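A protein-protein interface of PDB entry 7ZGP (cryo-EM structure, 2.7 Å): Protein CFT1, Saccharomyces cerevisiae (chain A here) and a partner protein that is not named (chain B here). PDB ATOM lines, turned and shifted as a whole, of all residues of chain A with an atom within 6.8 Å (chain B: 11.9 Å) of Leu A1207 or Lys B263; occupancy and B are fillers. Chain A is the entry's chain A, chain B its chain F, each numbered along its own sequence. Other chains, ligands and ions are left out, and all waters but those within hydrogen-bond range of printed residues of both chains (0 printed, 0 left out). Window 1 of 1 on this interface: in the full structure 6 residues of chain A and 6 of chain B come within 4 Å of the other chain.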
ATOM      1  N   SER A1161     -23.498 -20.874  10.579  1.00  0.00           N
ATOM      2  CA  SER A1161     -23.504 -21.477   9.249  1.00  0.00           C
ATOM      3  C   SER A1161     -22.288 -20.957   8.496  1.00  0.00           C
ATOM      4  O   SER A1161     -22.319 -19.900   7.867  1.00  0.00           O
ATOM      5  CB  SER A1161     -24.799 -21.156   8.515  1.00  0.00           C
ATOM      6  OG  SER A1161     -25.923 -21.633   9.235  1.00  0.00           O
ATOM      7  N   LEU A1162     -21.194 -21.717   8.564  1.00  0.00           N
ATOM      8  CA  LEU A1162     -19.952 -21.279   7.942  1.00  0.00           C
ATOM      9  C   LEU A1162     -19.990 -21.432   6.428  1.00  0.00           C
ATOM     10  O   LEU A1162     -19.359 -20.648   5.711  1.00  0.00           O
ATOM     11  CB  LEU A1162     -18.774 -22.054   8.528  1.00  0.00           C
ATOM     12  CG  LEU A1162     -18.533 -21.832  10.020  1.00  0.00           C
ATOM     13  CD1 LEU A1162     -17.445 -22.754  10.531  1.00  0.00           C
ATOM     14  CD2 LEU A1162     -18.177 -20.382  10.286  1.00  0.00           C
ATOM     15  N   ARG A1164     -21.781 -24.094   2.885  1.00  0.00           N
ATOM     16  CA  ARG A1164     -22.464 -25.287   2.409  1.00  0.00           C
ATOM     17  C   ARG A1164     -22.028 -25.571   0.981  1.00  0.00           C
ATOM     18  O   ARG A1164     -21.546 -24.686   0.271  1.00  0.00           O
ATOM     19  CB  ARG A1164     -23.987 -25.136   2.486  1.00  0.00           C
ATOM     20  CG  ARG A1164     -24.567 -24.182   1.465  1.00  0.00           C
ATOM     21  CD  ARG A1164     -25.705 -23.372   2.058  1.00  0.00           C
ATOM     22  NE  ARG A1164     -26.327 -22.495   1.072  1.00  0.00           N
ATOM     23  CZ  ARG A1164     -25.760 -21.407   0.570  1.00  0.00           C
ATOM     24  NH1 ARG A1164     -24.552 -21.017   0.944  1.00  0.00           N
ATOM     25  NH2 ARG A1164     -26.424 -20.689  -0.332  1.00  0.00           N
ATOM     26  N   ALA A1200     -12.934 -22.117   1.822  1.00  0.00           N
ATOM     27  CA  ALA A1200     -12.006 -21.115   1.304  1.00  0.00           C
ATOM     28  C   ALA A1200     -12.629 -19.736   1.460  1.00  0.00           C
ATOM     29  O   ALA A1200     -13.098 -19.139   0.482  1.00  0.00           O
ATOM     30  CB  ALA A1200     -11.648 -21.397  -0.155  1.00  0.00           C
ATOM     31  N   PRO A1201     -12.655 -19.200   2.683  1.00  0.00           N
ATOM     32  CA  PRO A1201     -13.192 -17.844   2.874  1.00  0.00           C
ATOM     33  C   PRO A1201     -12.396 -16.771   2.158  1.00  0.00           C
ATOM     34  O   PRO A1201     -12.953 -15.711   1.846  1.00  0.00           O
ATOM     35  CB  PRO A1201     -13.140 -17.659   4.395  1.00  0.00           C
ATOM     36  CG  PRO A1201     -12.084 -18.600   4.854  1.00  0.00           C
ATOM     37  CD  PRO A1201     -12.153 -19.781   3.939  1.00  0.00           C
ATOM     38  N   GLU A1203     -11.056 -17.040  -0.866  1.00  0.00           N
ATOM     39  CA  GLU A1203     -11.277 -17.055  -2.302  1.00  0.00           C
ATOM     40  C   GLU A1203     -12.291 -15.977  -2.688  1.00  0.00           C
ATOM     41  O   GLU A1203     -13.173 -15.633  -1.898  1.00  0.00           O
ATOM     42  CB  GLU A1203     -11.769 -18.425  -2.756  1.00  0.00           C
ATOM     43  CG  GLU A1203     -10.654 -19.418  -3.030  1.00  0.00           C
ATOM     44  CD  GLU A1203     -11.055 -20.487  -4.026  1.00  0.00           C
ATOM     45  OE1 GLU A1203     -12.203 -20.444  -4.516  1.00  0.00           O
ATOM     46  OE2 GLU A1203     -10.223 -21.371  -4.320  1.00  0.00           O
ATOM     47  N   PRO A1204     -12.179 -15.422  -3.901  1.00  0.00           N
ATOM     48  CA  PRO A1204     -13.052 -14.302  -4.282  1.00  0.00           C
ATOM     49  C   PRO A1204     -14.533 -14.654  -4.320  1.00  0.00           C
ATOM     50  O   PRO A1204     -15.339 -14.025  -3.628  1.00  0.00           O
ATOM     51  CB  PRO A1204     -12.540 -13.918  -5.677  1.00  0.00           C
ATOM     52  CG  PRO A1204     -11.796 -15.122  -6.164  1.00  0.00           C
ATOM     53  CD  PRO A1204     -11.187 -15.726  -4.944  1.00  0.00           C
ATOM     54  N   ASN A1205     -14.904 -15.652  -5.116  1.00  0.00           N
ATOM     55  CA  ASN A1205     -16.312 -16.014  -5.284  1.00  0.00           C
ATOM     56  C   ASN A1205     -16.737 -17.120  -4.324  1.00  0.00           C
ATOM     57  O   ASN A1205     -17.284 -18.145  -4.729  1.00  0.00           O
ATOM     58  CB  ASN A1205     -16.574 -16.416  -6.731  1.00  0.00           C
ATOM     59  CG  ASN A1205     -16.070 -15.387  -7.720  1.00  0.00           C
ATOM     60  OD1 ASN A1205     -15.606 -14.314  -7.334  1.00  0.00           O
ATOM     61  ND2 ASN A1205     -16.164 -15.706  -9.005  1.00  0.00           N
ATOM     62  N   SER A1206     -16.493 -16.916  -3.031  1.00  0.00           N
ATOM     63  CA  SER A1206     -16.928 -17.857  -2.011  1.00  0.00           C
ATOM     64  C   SER A1206     -17.923 -17.255  -1.032  1.00  0.00           C
ATOM     65  O   SER A1206     -18.428 -17.979  -0.167  1.00  0.00           O
ATOM     66  CB  SER A1206     -15.720 -18.406  -1.240  1.00  0.00           C
ATOM     67  OG  SER A1206     -14.996 -17.362  -0.615  1.00  0.00           O
ATOM     68  N   LEU A1207     -18.223 -15.962  -1.151  1.00  0.00           N
ATOM     69  CA  LEU A1207     -19.135 -15.259  -0.250  1.00  0.00           C
ATOM     70  C   LEU A1207     -18.698 -15.438   1.204  1.00  0.00           C
ATOM     71  O   LEU A1207     -19.447 -15.904   2.064  1.00  0.00           O
ATOM     72  CB  LEU A1207     -20.580 -15.722  -0.467  1.00  0.00           C
ATOM     73  CG  LEU A1207     -21.690 -14.887   0.175  1.00  0.00           C
ATOM     74  CD1 LEU A1207     -21.968 -13.647  -0.653  1.00  0.00           C
ATOM     75  CD2 LEU A1207     -22.954 -15.712   0.350  1.00  0.00           C
ATOM     76  N   SER A1208     -17.444 -15.059   1.459  1.00  0.00           N
ATOM     77  CA  SER A1208     -16.817 -15.216   2.773  1.00  0.00           C
ATOM     78  C   SER A1208     -16.874 -16.667   3.243  1.00  0.00           C
ATOM     79  O   SER A1208     -17.115 -16.951   4.418  1.00  0.00           O
ATOM     80  CB  SER A1208     -17.450 -14.282   3.806  1.00  0.00           C
ATOM     81  OG  SER A1208     -17.402 -12.935   3.373  1.00  0.00           O
ATOM     82  N   GLY A1209     -16.650 -17.595   2.315  1.00  0.00           N
ATOM     83  CA  GLY A1209     -16.645 -19.005   2.630  1.00  0.00           C
ATOM     84  C   GLY A1209     -18.002 -19.669   2.670  1.00  0.00           C
ATOM     85  O   GLY A1209     -18.070 -20.877   2.932  1.00  0.00           O
ATOM     86  N   GLN A1210     -19.086 -18.928   2.424  1.00  0.00           N
ATOM     87  CA  GLN A1210     -20.411 -19.535   2.460  1.00  0.00           C
ATOM     88  C   GLN A1210     -20.604 -20.535   1.329  1.00  0.00           C
ATOM     89  O   GLN A1210     -21.394 -21.477   1.466  1.00  0.00           O
ATOM     90  CB  GLN A1210     -21.488 -18.453   2.404  1.00  0.00           C
ATOM     91  CG  GLN A1210     -21.693 -17.725   3.717  1.00  0.00           C
ATOM     92  CD  GLN A1210     -22.298 -18.611   4.787  1.00  0.00           C
ATOM     93  OE1 GLN A1210     -22.996 -19.578   4.486  1.00  0.00           O
ATOM     94  NE2 GLN A1210     -22.030 -18.285   6.045  1.00  0.00           N
ATOM     95  N   ARG A1211     -19.902 -20.355   0.216  1.00  0.00           N
ATOM     96  CA  ARG A1211     -19.937 -21.295  -0.896  1.00  0.00           C
ATOM     97  C   ARG A1211     -18.687 -22.162  -0.826  1.00  0.00           C
ATOM     98  O   ARG A1211     -17.574 -21.674  -1.048  1.00  0.00           O
ATOM     99  CB  ARG A1211     -20.020 -20.561  -2.232  1.00  0.00           C
ATOM    100  CG  ARG A1211     -21.195 -19.609  -2.355  1.00  0.00           C
ATOM    101  CD  ARG A1211     -21.467 -19.262  -3.811  1.00  0.00           C
ATOM    102  NE  ARG A1211     -21.082 -17.895  -4.136  1.00  0.00           N
ATOM    103  CZ  ARG A1211     -21.801 -16.821  -3.839  1.00  0.00           C
ATOM    104  NH1 ARG A1211     -22.958 -16.917  -3.205  1.00  0.00           N
ATOM    105  NH2 ARG A1211     -21.349 -15.620  -4.189  1.00  0.00           N
ATOM    106  N   GLN B 255     -29.353  -2.917   5.721  1.00  0.00           N
ATOM    107  CA  GLN B 255     -28.219  -3.342   6.579  1.00  0.00           C
ATOM    108  C   GLN B 255     -27.906  -4.791   6.211  1.00  0.00           C
ATOM    109  O   GLN B 255     -26.722  -5.106   6.007  1.00  0.00           O
ATOM    110  CB  GLN B 255     -28.581  -3.206   8.057  1.00  0.00           C
ATOM    111  CG  GLN B 255     -27.494  -3.714   8.994  1.00  0.00           C
ATOM    112  CD  GLN B 255     -27.882  -3.577  10.445  1.00  0.00           C
ATOM    113  OE1 GLN B 255     -28.976  -3.123  10.775  1.00  0.00           O
ATOM    114  NE2 GLN B 255     -26.980  -3.970  11.330  1.00  0.00           N
ATOM    115  N   SER B 256     -28.942  -5.625   6.108  1.00  0.00           N
ATOM    116  CA  SER B 256     -28.743  -7.033   5.683  1.00  0.00           C
ATOM    117  C   SER B 256     -28.198  -7.048   4.254  1.00  0.00           C
ATOM    118  O   SER B 256     -27.281  -7.843   3.980  1.00  0.00           O
ATOM    119  CB  SER B 256     -30.025  -7.812   5.790  1.00  0.00           C
ATOM    120  OG  SER B 256     -30.516  -7.790   7.122  1.00  0.00           O
ATOM    121  N   TRP B 257     -28.737  -6.188   3.388  1.00  0.00           N
ATOM    122  CA  TRP B 257     -28.243  -6.104   1.989  1.00  0.00           C
ATOM    123  C   TRP B 257     -26.785  -5.640   2.001  1.00  0.00           C
ATOM    124  O   TRP B 257     -25.985  -6.194   1.228  1.00  0.00           O
ATOM    125  CB  TRP B 257     -29.125  -5.173   1.151  1.00  0.00           C
ATOM    126  CG  TRP B 257     -28.814  -5.214  -0.312  1.00  0.00           C
ATOM    127  CD1 TRP B 257     -28.238  -4.230  -1.061  1.00  0.00           C
ATOM    128  CD2 TRP B 257     -29.053  -6.311  -1.210  1.00  0.00           C
ATOM    129  NE1 TRP B 257     -28.109  -4.635  -2.362  1.00  0.00           N
ATOM    130  CE2 TRP B 257     -28.600  -5.908  -2.484  1.00  0.00           C
ATOM    131  CE3 TRP B 257     -29.606  -7.588  -1.064  1.00  0.00           C
ATOM    132  CZ2 TRP B 257     -28.684  -6.739  -3.600  1.00  0.00           C
ATOM    133  CZ3 TRP B 257     -29.689  -8.408  -2.167  1.00  0.00           C
ATOM    134  CH2 TRP B 257     -29.234  -7.986  -3.416  1.00  0.00           C
ATOM    135  N   GLU B 258     -26.463  -4.665   2.855  1.00  0.00           N
ATOM    136  CA  GLU B 258     -25.072  -4.150   2.950  1.00  0.00           C
ATOM    137  C   GLU B 258     -24.151  -5.270   3.440  1.00  0.00           C
ATOM    138  O   GLU B 258     -23.074  -5.443   2.847  1.00  0.00           O
ATOM    139  CB  GLU B 258     -25.022  -2.939   3.880  1.00  0.00           C
ATOM    140  CG  GLU B 258     -25.825  -1.759   3.367  1.00  0.00           C
ATOM    141  CD  GLU B 258     -25.690  -0.495   4.199  1.00  0.00           C
ATOM    142  OE1 GLU B 258     -25.018  -0.551   5.247  1.00  0.00           O
ATOM    143  OE2 GLU B 258     -26.256   0.539   3.795  1.00  0.00           O
ATOM    144  N   ASP B 259     -24.567  -6.000   4.478  1.00  0.00           N
ATOM    145  CA  ASP B 259     -23.762  -7.144   4.981  1.00  0.00           C
ATOM    146  C   ASP B 259     -23.530  -8.115   3.823  1.00  0.00           C
ATOM    147  O   ASP B 259     -22.392  -8.588   3.668  1.00  0.00           O
ATOM    148  CB  ASP B 259     -24.444  -7.814   6.174  1.00  0.00           C
ATOM    149  CG  ASP B 259     -24.711  -6.857   7.323  1.00  0.00           C
ATOM    150  OD1 ASP B 259     -24.230  -5.708   7.251  1.00  0.00           O
ATOM    151  OD2 ASP B 259     -25.403  -7.264   8.276  1.00  0.00           O
ATOM    152  N   TYR B 260     -24.575  -8.391   3.041  1.00  0.00           N
ATOM    153  CA  TYR B 260     -24.452  -9.283   1.863  1.00  0.00           C
ATOM    154  C   TYR B 260     -23.388  -8.698   0.936  1.00  0.00           C
ATOM    155  O   TYR B 260     -22.569  -9.467   0.395  1.00  0.00           O
ATOM    156  CB  TYR B 260     -25.799  -9.420   1.154  1.00  0.00           C
ATOM    157  CG  TYR B 260     -25.718  -9.913  -0.268  1.00  0.00           C
ATOM    158  CD1 TYR B 260     -25.252 -11.183  -0.560  1.00  0.00           C
ATOM    159  CD2 TYR B 260     -26.118  -9.111  -1.324  1.00  0.00           C
ATOM    160  CE1 TYR B 260     -25.178 -11.643  -1.863  1.00  0.00           C
ATOM    161  CE2 TYR B 260     -26.052  -9.555  -2.633  1.00  0.00           C
ATOM    162  CZ  TYR B 260     -25.581 -10.827  -2.904  1.00  0.00           C
ATOM    163  OH  TYR B 260     -25.512 -11.273  -4.192  1.00  0.00           O
ATOM    164  N   GLN B 261     -23.402  -7.374   0.770  1.00  0.00           N
ATOM    165  CA  GLN B 261     -22.388  -6.703  -0.079  1.00  0.00           C
ATOM    166  C   GLN B 261     -21.015  -6.891   0.571  1.00  0.00           C
ATOM    167  O   GLN B 261     -20.074  -7.295  -0.142  1.00  0.00           O
ATOM    168  CB  GLN B 261     -22.732  -5.223  -0.250  1.00  0.00           C
ATOM    169  CG  GLN B 261     -24.119  -4.987  -0.824  1.00  0.00           C
ATOM    170  CD  GLN B 261     -24.315  -5.687  -2.146  1.00  0.00           C
ATOM    171  OE1 GLN B 261     -23.385  -5.842  -2.935  1.00  0.00           O
ATOM    172  NE2 GLN B 261     -25.541  -6.110  -2.403  1.00  0.00           N
ATOM    173  N   ARG B 262     -20.918  -6.629   1.879  1.00  0.00           N
ATOM    174  CA  ARG B 262     -19.639  -6.805   2.558  1.00  0.00           C
ATOM    175  C   ARG B 262     -19.133  -8.234   2.425  1.00  0.00           C
ATOM    176  O   ARG B 262     -17.946  -8.459   2.162  1.00  0.00           O
ATOM    177  CB  ARG B 262     -19.779  -6.425   4.031  1.00  0.00           C
ATOM    178  CG  ARG B 262     -18.496  -6.525   4.823  1.00  0.00           C
ATOM    179  CD  ARG B 262     -18.706  -6.090   6.266  1.00  0.00           C
ATOM    180  NE  ARG B 262     -19.765  -6.839   6.936  1.00  0.00           N
ATOM    181  CZ  ARG B 262     -19.735  -8.141   7.189  1.00  0.00           C
ATOM    182  NH1 ARG B 262     -18.691  -8.887   6.865  1.00  0.00           N
ATOM    183  NH2 ARG B 262     -20.774  -8.708   7.793  1.00  0.00           N
ATOM    184  N   LYS B 263     -20.020  -9.214   2.604  1.00  0.00           N
ATOM    185  CA  LYS B 263     -19.625 -10.611   2.484  1.00  0.00           C
ATOM    186  C   LYS B 263     -19.309 -10.997   1.046  1.00  0.00           C
ATOM    187  O   LYS B 263     -18.599 -11.983   0.825  1.00  0.00           O
ATOM    188  CB  LYS B 263     -20.723 -11.515   3.045  1.00  0.00           C
ATOM    189  CG  LYS B 263     -20.839 -11.466   4.561  1.00  0.00           C
ATOM    190  CD  LYS B 263     -21.594 -12.666   5.106  1.00  0.00           C
ATOM    191  CE  LYS B 263     -20.659 -13.609   5.844  1.00  0.00           C
ATOM    192  NZ  LYS B 263     -20.930 -15.035   5.517  1.00  0.00           N
ATOM    193  N   ARG B 264     -19.820 -10.249   0.066  1.00  0.00           N
ATOM    194  CA  ARG B 264     -19.451 -10.494  -1.322  1.00  0.00           C
ATOM    195  C   ARG B 264     -18.014 -10.087  -1.617  1.00  0.00           C
ATOM    196  O   ARG B 264     -17.458 -10.518  -2.633  1.00  0.00           O
ATOM    197  CB  ARG B 264     -20.398  -9.751  -2.262  1.00  0.00           C
ATOM    198  CG  ARG B 264     -21.600 -10.560  -2.707  1.00  0.00           C
ATOM    199  CD  ARG B 264     -22.377  -9.823  -3.782  1.00  0.00           C
ATOM    200  NE  ARG B 264     -21.500  -9.285  -4.814  1.00  0.00           N
ATOM    201  CZ  ARG B 264     -21.125  -9.948  -5.899  1.00  0.00           C
ATOM    202  NH1 ARG B 264     -21.537 -11.184  -6.130  1.00  0.00           N
ATOM    203  NH2 ARG B 264     -20.320  -9.355  -6.775  1.00  0.00           N
ATOM    204  N   GLU B 265     -17.406  -9.269  -0.762  1.00  0.00           N
ATOM    205  CA  GLU B 265     -16.033  -8.841  -0.976  1.00  0.00           C
ATOM    206  C   GLU B 265     -15.067  -9.995  -0.720  1.00  0.00           C
ATOM    207  O   GLU B 265     -15.360 -10.937   0.020  1.00  0.00           O
ATOM    208  CB  GLU B 265     -15.691  -7.658  -0.071  1.00  0.00           C
ATOM    209  CG  GLU B 265     -16.649  -6.483  -0.190  1.00  0.00           C
ATOM    210  CD  GLU B 265     -16.766  -5.960  -1.609  1.00  0.00           C
ATOM    211  OE1 GLU B 265     -15.934  -5.116  -2.002  1.00  0.00           O
ATOM    212  OE2 GLU B 265     -17.692  -6.387  -2.330  1.00  0.00           O
ATOM    213  N   ASN B 266     -13.898  -9.908  -1.349  1.00  0.00           N
ATOM    214  CA  ASN B 266     -12.907 -10.969  -1.235  1.00  0.00           C
ATOM    215  C   ASN B 266     -12.282 -10.969   0.153  1.00  0.00           C
ATOM    216  O   ASN B 266     -11.843  -9.925   0.649  1.00  0.00           O
ATOM    217  CB  ASN B 266     -11.827 -10.797  -2.302  1.00  0.00           C
ATOM    218  CG  ASN B 266     -12.393 -10.777  -3.707  1.00  0.00           C
ATOM    219  OD1 ASN B 266     -13.609 -10.732  -3.898  1.00  0.00           O
ATOM    220  ND2 ASN B 266     -11.512 -10.806  -4.699  1.00  0.00           N
ATOM    221  N   ARG B 267     -12.251 -12.143   0.782  1.00  0.00           N
ATOM    222  CA  ARG B 267     -11.641 -12.371   2.089  1.00  0.00           C
ATOM    223  C   ARG B 267     -12.264 -11.524   3.193  1.00  0.00           C
ATOM    224  O   ARG B 267     -11.609 -11.262   4.209  1.00  0.00           O
ATOM    225  CB  ARG B 267     -10.125 -12.137   2.050  1.00  0.00           C
ATOM    226  N   GLN B 268     -13.507 -11.088   3.027  1.00  0.00           N
ATOM    227  CA  GLN B 268     -14.137 -10.208   4.003  1.00  0.00           C
ATOM    228  C   GLN B 268     -15.296 -10.900   4.710  1.00  0.00           C
ATOM    229  O   GLN B 268     -15.229 -11.166   5.910  1.00  0.00           O
ATOM    230  CB  GLN B 268     -14.621  -8.923   3.326  1.00  0.00           C
ATOM    231  CG  GLN B 268     -14.984  -7.807   4.290  1.00  0.00           C
ATOM    232  CD  GLN B 268     -14.808  -6.434   3.673  1.00  0.00           C
ATOM    233  OE1 GLN B 268     -14.069  -6.270   2.702  1.00  0.00           O
ATOM    234  NE2 GLN B 268     -15.477  -5.438   4.239  1.00  0.00           N
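Printed residues of chain A that touch a printed residue of chain B: Pro A1201, Pro A1204, Leu A1207, Ser A1208 and Gln A1210. Hydrophobic or aromatic side chains of chain A within 4 Å of the printed part of chain B: Pro A1204 and Leu A1207. Along chain A the printed residues that touch a printed residue of chain B span positions 1201 to 1210. Of the 14 printed residues of chain B, 6 touch a printed residue of chain A. Hydrophobic or aromatic side chains of chain B within 4 Å of the printed part of chain A: Tyr B260. Among the printed residues, no Asp or Glu carboxylate lies within 4 Å of a Lys or Arg side-chain nitrogen of the other chain.
O of Lys B263 is in hydrogen-bond range of OG of Ser A1208 (3.0 Å). The side-chain amino group (NZ) of Lys B263 lies close to the side-chain amide nitrogen (NE2) of Gln A1210, 3.5 Å away.
Pro A1201 touches Arg B267 (O to CA, 3.6 Å). Pro A1204 touches Asn B266 (CB to ND2, 3.4 Å). CD1 of Leu A1207 touches CE1 of Tyr B260, at 3.97 Å. Leu A1207 touches Lys B263 (C to O, 3.5 Å). Leu A1207 touches Arg B264. Ser A1208 touches Gln B268.
Of chain B, only Tyr B260, Lys B263 and Arg B264 come within 4 Å of Leu A1207. Lys B263 touches just these residues of chain A: Leu A1207, Ser A1208 and Gln A1210. Ser A1206 touches none of the printed residues of chain B. No residue of chain B comes within 4 Å of Gly A1209. Of the printed residues of chain A, Arg B264 touches Leu A1207 (3.7 Å). Of the printed residues of chain A, Arg B267 touches Pro A1201 (3.6 Å). The nearest residue of chain A that does not touch Lys B263 is Ser A1161 (5.6 Å). The nearest printed residue of chain A that does not touch Gln B268 is Pro A1201 (4.8 Å).
The backbone carbonyl oxygen (O) of Gln A1210 is in hydrogen-bond range of the backbone NH (N) of Arg A1164. The backbone carbonyl oxygen (O) of Ser A1161 sits at hydrogen-bond distance from the side-chain amide nitrogen (NE2) of Gln A1210 (2.5 Å).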
